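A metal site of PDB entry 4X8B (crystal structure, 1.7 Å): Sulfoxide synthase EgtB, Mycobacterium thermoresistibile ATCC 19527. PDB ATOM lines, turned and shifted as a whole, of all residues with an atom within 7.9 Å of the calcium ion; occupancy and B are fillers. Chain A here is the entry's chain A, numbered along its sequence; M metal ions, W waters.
N of Gly 357 is in hydrogen-bond range of O of Gly 399, 2.9 Å away. The side-chain sulfur (SD) of Met 355 sits at hydrogen-bond distance from the guanidinium group (NE) of Arg 429, 3.3 Å away. The backbone carbonyl oxygen (O) of Gly 400 is in hydrogen-bond range of the backbone NH (N) of Trp 360. The backbone carbonyl oxygen (O) of Glu 361 sits at hydrogen-bond distance from the backbone NH (N) of Arg 398 (2.9 Å). NE1 of Trp 300 is in hydrogen-bond range of OE1 of Glu 361. The side-chain carboxylate (OE1) of Glu 361 lies within salt-bridge range of the guanidinium group (NE) of Arg 429, 2.7 Å away. OD2 of Asp 358 sits at hydrogen-bond distance from NE2 of Gln 354. O of Gln 354 is in hydrogen-bond range of NH2 of Arg 429 (3.1 Å).
Gln 354 touches the calcium ion. OE2 of Glu 361 touches the calcium ion, at 3.2 Å. O of Gly 399 touches the calcium ion (3.5 Å). Along chain A the residues within 4 Å of the calcium ion span positions 354 to 400.
The calcium ion is bound by O of Val 359 (2.6 Å), O of Gly 357 (2.6 Å) and O of Met 355 (2.7 Å). The calcium ion has three donor atoms within binding distance. Slightly farther from the calcium ion lies the backbone carbonyl oxygen (O) of Gly 400 (2.9 Å). Slightly farther from the calcium ion lies water W1 (3.0 Å).
Water W1 lies within hydrogen-bond range of OE2 of Glu 361, O of Gln 354 and N of Val 359.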
ATOM      1  N   PRO A 214      29.011   3.572 -16.055  1.00  0.00           N
ATOM      2  CA  PRO A 214      29.641   3.293 -17.350  1.00  0.00           C
ATOM      3  C   PRO A 214      30.096   4.538 -18.098  1.00  0.00           C
ATOM      4  O   PRO A 214      29.648   5.651 -17.824  1.00  0.00           O
ATOM      5  CB  PRO A 214      28.521   2.595 -18.141  1.00  0.00           C
ATOM      6  CG  PRO A 214      27.655   1.962 -17.076  1.00  0.00           C
ATOM      7  CD  PRO A 214      27.640   3.025 -15.993  1.00  0.00           C
ATOM      8  N   TRP A 300      35.325  -6.944 -11.123  1.00  0.00           N
ATOM      9  CA  TRP A 300      33.965  -6.515 -11.362  1.00  0.00           C
ATOM     10  C   TRP A 300      33.036  -7.094 -10.293  1.00  0.00           C
ATOM     11  O   TRP A 300      32.246  -6.384  -9.669  1.00  0.00           O
ATOM     12  CB  TRP A 300      33.525  -6.928 -12.789  1.00  0.00           C
ATOM     13  CG  TRP A 300      32.249  -6.286 -13.174  1.00  0.00           C
ATOM     14  CD1 TRP A 300      32.086  -5.173 -13.962  1.00  0.00           C
ATOM     15  CD2 TRP A 300      30.934  -6.694 -12.779  1.00  0.00           C
ATOM     16  NE1 TRP A 300      30.745  -4.864 -14.072  1.00  0.00           N
ATOM     17  CE2 TRP A 300      30.020  -5.787 -13.362  1.00  0.00           C
ATOM     18  CE3 TRP A 300      30.441  -7.749 -11.999  1.00  0.00           C
ATOM     19  CZ2 TRP A 300      28.640  -5.872 -13.140  1.00  0.00           C
ATOM     20  CZ3 TRP A 300      29.054  -7.837 -11.789  1.00  0.00           C
ATOM     21  CH2 TRP A 300      28.193  -6.903 -12.360  1.00  0.00           C
ATOM     22  N   ASN A 329      17.484  -0.963 -14.314  1.00  0.00           N
ATOM     23  CA  ASN A 329      16.838  -1.042 -15.620  1.00  0.00           C
ATOM     24  C   ASN A 329      17.041  -2.418 -16.252  1.00  0.00           C
ATOM     25  O   ASN A 329      18.080  -2.700 -16.836  1.00  0.00           O
ATOM     26  CB  ASN A 329      17.412   0.060 -16.523  1.00  0.00           C
ATOM     27  CG  ASN A 329      16.860   0.034 -17.929  1.00  0.00           C
ATOM     28  OD1 ASN A 329      15.751  -0.479 -18.183  1.00  0.00           O
ATOM     29  ND2 ASN A 329      17.618   0.602 -18.866  1.00  0.00           N
ATOM     30  N   LEU A 330      16.014  -3.251 -16.103  1.00  0.00           N
ATOM     31  CA  LEU A 330      16.032  -4.653 -16.482  1.00  0.00           C
ATOM     32  C   LEU A 330      14.739  -5.020 -17.195  1.00  0.00           C
ATOM     33  O   LEU A 330      13.757  -4.287 -17.094  1.00  0.00           O
ATOM     34  CB  LEU A 330      16.189  -5.531 -15.243  1.00  0.00           C
ATOM     35  CG  LEU A 330      17.584  -5.431 -14.586  1.00  0.00           C
ATOM     36  CD1 LEU A 330      17.533  -6.024 -13.193  1.00  0.00           C
ATOM     37  CD2 LEU A 330      18.646  -6.124 -15.409  1.00  0.00           C
ATOM     38  N   GLU A 353      27.484   2.315  -9.400  1.00  0.00           N
ATOM     39  CA  GLU A 353      26.071   2.378  -9.805  1.00  0.00           C
ATOM     40  C   GLU A 353      25.838   1.709 -11.159  1.00  0.00           C
ATOM     41  O   GLU A 353      26.749   1.650 -12.003  1.00  0.00           O
ATOM     42  CB  GLU A 353      25.594   3.831  -9.870  1.00  0.00           C
ATOM     43  CG  GLU A 353      25.689   4.491  -8.479  1.00  0.00           C
ATOM     44  CD  GLU A 353      25.115   5.896  -8.393  1.00  0.00           C
ATOM     45  OE1 GLU A 353      24.335   6.326  -9.270  1.00  0.00           O
ATOM     46  OE2 GLU A 353      25.423   6.568  -7.392  1.00  0.00           O
ATOM     47  N   GLN A 354      24.616   1.220 -11.338  1.00  0.00           N
ATOM     48  CA  GLN A 354      24.162   0.608 -12.572  1.00  0.00           C
ATOM     49  C   GLN A 354      25.000  -0.582 -12.964  1.00  0.00           C
ATOM     50  O   GLN A 354      25.205  -0.900 -14.148  1.00  0.00           O
ATOM     51  CB  GLN A 354      24.098   1.685 -13.665  1.00  0.00           C
ATOM     52  CG  GLN A 354      22.925   2.644 -13.407  1.00  0.00           C
ATOM     53  CD  GLN A 354      23.003   3.903 -14.229  1.00  0.00           C
ATOM     54  OE1 GLN A 354      23.674   4.867 -13.860  1.00  0.00           O
ATOM     55  NE2 GLN A 354      22.318   3.911 -15.359  1.00  0.00           N
ATOM     56  N   MET A 355      25.495  -1.290 -11.960  1.00  0.00           N
ATOM     57  CA  MET A 355      26.225  -2.532 -12.194  1.00  0.00           C
ATOM     58  C   MET A 355      25.302  -3.602 -12.759  1.00  0.00           C
ATOM     59  O   MET A 355      25.689  -4.354 -13.658  1.00  0.00           O
ATOM     60  CB  MET A 355      26.874  -3.020 -10.885  1.00  0.00           C
ATOM     61  CG  MET A 355      27.969  -2.091 -10.390  1.00  0.00           C
ATOM     62  SD  MET A 355      29.445  -2.253 -11.411  1.00  0.00           S
ATOM     63  CE  MET A 355      30.262  -3.683 -10.695  1.00  0.00           C
ATOM     64  N   LEU A 356      24.093  -3.691 -12.216  1.00  0.00           N
ATOM     65  CA  LEU A 356      23.098  -4.596 -12.800  1.00  0.00           C
ATOM     66  C   LEU A 356      22.167  -3.819 -13.748  1.00  0.00           C
ATOM     67  O   LEU A 356      21.673  -2.738 -13.423  1.00  0.00           O
ATOM     68  CB  LEU A 356      22.270  -5.343 -11.735  1.00  0.00           C
ATOM     69  CG  LEU A 356      23.056  -6.282 -10.812  1.00  0.00           C
ATOM     70  CD1 LEU A 356      22.038  -7.123 -10.031  1.00  0.00           C
ATOM     71  CD2 LEU A 356      24.051  -7.177 -11.527  1.00  0.00           C
ATOM     72  N   GLY A 357      21.937  -4.398 -14.926  1.00  0.00           N
ATOM     73  CA  GLY A 357      21.112  -3.740 -15.929  1.00  0.00           C
ATOM     74  C   GLY A 357      21.868  -2.732 -16.745  1.00  0.00           C
ATOM     75  O   GLY A 357      23.081  -2.552 -16.598  1.00  0.00           O
ATOM     76  N   ASP A 358      21.115  -2.062 -17.617  1.00  0.00           N
ATOM     77  CA  ASP A 358      21.606  -1.042 -18.562  1.00  0.00           C
ATOM     78  C   ASP A 358      22.487  -1.636 -19.658  1.00  0.00           C
ATOM     79  O   ASP A 358      21.934  -1.940 -20.732  1.00  0.00           O
ATOM     80  CB  ASP A 358      22.273   0.101 -17.803  1.00  0.00           C
ATOM     81  CG  ASP A 358      21.240   0.980 -17.128  1.00  0.00           C
ATOM     82  OD1 ASP A 358      20.241   1.369 -17.812  1.00  0.00           O
ATOM     83  OD2 ASP A 358      21.388   1.285 -15.907  1.00  0.00           O
ATOM     84  N   VAL A 359      23.796  -1.853 -19.453  1.00  0.00           N
ATOM     85  CA  VAL A 359      24.592  -2.531 -20.488  1.00  0.00           C
ATOM     86  C   VAL A 359      25.446  -3.646 -19.908  1.00  0.00           C
ATOM     87  O   VAL A 359      25.938  -3.557 -18.785  1.00  0.00           O
ATOM     88  CB  VAL A 359      25.524  -1.560 -21.270  1.00  0.00           C
ATOM     89  CG1 VAL A 359      24.714  -0.579 -22.106  1.00  0.00           C
ATOM     90  CG2 VAL A 359      26.475  -0.810 -20.346  1.00  0.00           C
ATOM     91  N   TRP A 360      25.585  -4.728 -20.681  1.00  0.00           N
ATOM     92  CA  TRP A 360      26.630  -5.704 -20.405  1.00  0.00           C
ATOM     93  C   TRP A 360      27.974  -4.995 -20.444  1.00  0.00           C
ATOM     94  O   TRP A 360      28.212  -4.196 -21.337  1.00  0.00           O
ATOM     95  CB  TRP A 360      26.655  -6.842 -21.423  1.00  0.00           C
ATOM     96  CG  TRP A 360      25.510  -7.828 -21.292  1.00  0.00           C
ATOM     97  CD1 TRP A 360      24.402  -7.935 -22.094  1.00  0.00           C
ATOM     98  CD2 TRP A 360      25.393  -8.865 -20.306  1.00  0.00           C
ATOM     99  NE1 TRP A 360      23.599  -8.946 -21.650  1.00  0.00           N
ATOM    100  CE2 TRP A 360      24.188  -9.545 -20.562  1.00  0.00           C
ATOM    101  CE3 TRP A 360      26.183  -9.285 -19.219  1.00  0.00           C
ATOM    102  CZ2 TRP A 360      23.741 -10.616 -19.771  1.00  0.00           C
ATOM    103  CZ3 TRP A 360      25.764 -10.319 -18.463  1.00  0.00           C
ATOM    104  CH2 TRP A 360      24.545 -10.983 -18.723  1.00  0.00           C
ATOM    105  N   GLU A 361      28.834  -5.308 -19.475  1.00  0.00           N
ATOM    106  CA  GLU A 361      30.118  -4.605 -19.353  1.00  0.00           C
ATOM    107  C   GLU A 361      31.280  -5.538 -19.646  1.00  0.00           C
ATOM    108  O   GLU A 361      31.446  -6.579 -19.011  1.00  0.00           O
ATOM    109  CB  GLU A 361      30.232  -3.970 -17.957  1.00  0.00           C
ATOM    110  CG  GLU A 361      29.139  -2.917 -17.752  1.00  0.00           C
ATOM    111  CD  GLU A 361      29.035  -2.390 -16.337  1.00  0.00           C
ATOM    112  OE1 GLU A 361      29.976  -2.563 -15.493  1.00  0.00           O
ATOM    113  OE2 GLU A 361      27.986  -1.739 -16.077  1.00  0.00           O
ATOM    114  N   ARG A 398      29.814  -8.724 -17.851  1.00  0.00           N
ATOM    115  CA  ARG A 398      29.093  -8.811 -16.577  1.00  0.00           C
ATOM    116  C   ARG A 398      27.960  -7.827 -16.423  1.00  0.00           C
ATOM    117  O   ARG A 398      27.904  -6.766 -17.092  1.00  0.00           O
ATOM    118  CB  ARG A 398      30.077  -8.607 -15.405  1.00  0.00           C
ATOM    119  CG  ARG A 398      31.160  -9.720 -15.273  1.00  0.00           C
ATOM    120  CD  ARG A 398      30.541 -11.136 -15.203  1.00  0.00           C
ATOM    121  NE  ARG A 398      31.422 -12.051 -14.473  1.00  0.00           N
ATOM    122  CZ  ARG A 398      31.370 -12.262 -13.155  1.00  0.00           C
ATOM    123  NH1 ARG A 398      30.440 -11.672 -12.422  1.00  0.00           N
ATOM    124  NH2 ARG A 398      32.255 -13.074 -12.580  1.00  0.00           N
ATOM    125  N   GLY A 399      27.025  -8.182 -15.541  1.00  0.00           N
ATOM    126  CA  GLY A 399      26.074  -7.243 -14.969  1.00  0.00           C
ATOM    127  C   GLY A 399      24.722  -7.163 -15.648  1.00  0.00           C
ATOM    128  O   GLY A 399      23.810  -6.573 -15.116  1.00  0.00           O
ATOM    129  N   GLY A 400      24.584  -7.775 -16.803  1.00  0.00           N
ATOM    130  CA  GLY A 400      23.338  -7.728 -17.516  1.00  0.00           C
ATOM    131  C   GLY A 400      23.124  -6.415 -18.236  1.00  0.00           C
ATOM    132  O   GLY A 400      23.709  -5.396 -17.900  1.00  0.00           O
ATOM    133  N   SER A 401      22.243  -6.424 -19.209  1.00  0.00           N
ATOM    134  CA  SER A 401      21.812  -5.219 -19.911  1.00  0.00           C
ATOM    135  C   SER A 401      20.351  -4.898 -19.556  1.00  0.00           C
ATOM    136  O   SER A 401      19.690  -5.620 -18.810  1.00  0.00           O
ATOM    137  CB  SER A 401      21.901  -5.410 -21.413  1.00  0.00           C
ATOM    138  OG  SER A 401      20.877  -6.307 -21.798  1.00  0.00           O
ATOM    139  N   TRP A 402      19.842  -3.825 -20.163  1.00  0.00           N
ATOM    140  CA  TRP A 402      18.441  -3.455 -20.072  1.00  0.00           C
ATOM    141  C   TRP A 402      17.505  -4.553 -20.547  1.00  0.00           C
ATOM    142  O   TRP A 402      16.315  -4.548 -20.205  1.00  0.00           O
ATOM    143  CB  TRP A 402      18.182  -2.164 -20.885  1.00  0.00           C
ATOM    144  CG  TRP A 402      18.494  -2.317 -22.373  1.00  0.00           C
ATOM    145  CD1 TRP A 402      19.619  -1.904 -23.012  1.00  0.00           C
ATOM    146  CD2 TRP A 402      17.682  -2.946 -23.366  1.00  0.00           C
ATOM    147  NE1 TRP A 402      19.566  -2.242 -24.353  1.00  0.00           N
ATOM    148  CE2 TRP A 402      18.378  -2.884 -24.595  1.00  0.00           C
ATOM    149  CE3 TRP A 402      16.427  -3.555 -23.337  1.00  0.00           C
ATOM    150  CZ2 TRP A 402      17.865  -3.435 -25.761  1.00  0.00           C
ATOM    151  CZ3 TRP A 402      15.932  -4.099 -24.499  1.00  0.00           C
ATOM    152  CH2 TRP A 402      16.651  -4.038 -25.690  1.00  0.00           C
ATOM    153  N   LEU A 409      19.152 -12.981 -13.339  1.00  0.00           N
ATOM    154  CA  LEU A 409      20.394 -12.213 -13.177  1.00  0.00           C
ATOM    155  C   LEU A 409      20.883 -12.161 -11.726  1.00  0.00           C
ATOM    156  O   LEU A 409      20.080 -11.998 -10.804  1.00  0.00           O
ATOM    157  CB  LEU A 409      20.201 -10.792 -13.687  1.00  0.00           C
ATOM    158  CG  LEU A 409      21.426  -9.854 -13.685  1.00  0.00           C
ATOM    159  CD1 LEU A 409      22.527 -10.365 -14.602  1.00  0.00           C
ATOM    160  CD2 LEU A 409      20.961  -8.455 -14.076  1.00  0.00           C
ATOM    161  N   PHE A 425      24.208  -6.068 -26.471  1.00  0.00           N
ATOM    162  CA  PHE A 425      23.927  -4.786 -25.785  1.00  0.00           C
ATOM    163  C   PHE A 425      25.015  -4.539 -24.742  1.00  0.00           C
ATOM    164  O   PHE A 425      24.802  -4.651 -23.516  1.00  0.00           O
ATOM    165  CB  PHE A 425      22.498  -4.803 -25.194  1.00  0.00           C
ATOM    166  CG  PHE A 425      21.437  -5.072 -26.231  1.00  0.00           C
ATOM    167  CD1 PHE A 425      21.250  -4.178 -27.282  1.00  0.00           C
ATOM    168  CD2 PHE A 425      20.665  -6.224 -26.201  1.00  0.00           C
ATOM    169  CE1 PHE A 425      20.310  -4.417 -28.279  1.00  0.00           C
ATOM    170  CE2 PHE A 425      19.730  -6.473 -27.207  1.00  0.00           C
ATOM    171  CZ  PHE A 425      19.544  -5.566 -28.237  1.00  0.00           C
ATOM    172  N   GLY A 427      28.549  -2.396 -23.313  1.00  0.00           N
ATOM    173  CA  GLY A 427      29.311  -1.177 -23.129  1.00  0.00           C
ATOM    174  C   GLY A 427      30.525  -1.400 -22.268  1.00  0.00           C
ATOM    175  O   GLY A 427      31.110  -2.507 -22.229  1.00  0.00           O
ATOM    176  N   ARG A 429      32.775  -0.141 -18.579  1.00  0.00           N
ATOM    177  CA  ARG A 429      33.057   0.504 -17.306  1.00  0.00           C
ATOM    178  C   ARG A 429      34.562   0.434 -17.084  1.00  0.00           C
ATOM    179  O   ARG A 429      35.174  -0.630 -17.255  1.00  0.00           O
ATOM    180  CB  ARG A 429      32.326  -0.152 -16.145  1.00  0.00           C
ATOM    181  CG  ARG A 429      32.510   0.542 -14.804  1.00  0.00           C
ATOM    182  CD  ARG A 429      31.835  -0.204 -13.660  1.00  0.00           C
ATOM    183  NE  ARG A 429      30.413  -0.407 -13.942  1.00  0.00           N
ATOM    184  CZ  ARG A 429      29.418   0.310 -13.462  1.00  0.00           C
ATOM    185  NH1 ARG A 429      29.642   1.303 -12.597  1.00  0.00           N
ATOM    186  NH2 ARG A 429      28.181   0.001 -13.821  1.00  0.00           N
HETATM  187 CA    CA M   1      25.396  -3.665 -16.281  1.00  0.00          CA
HETATM  188  O   HOH W   1      25.568  -0.759 -16.975  1.00  0.00           O
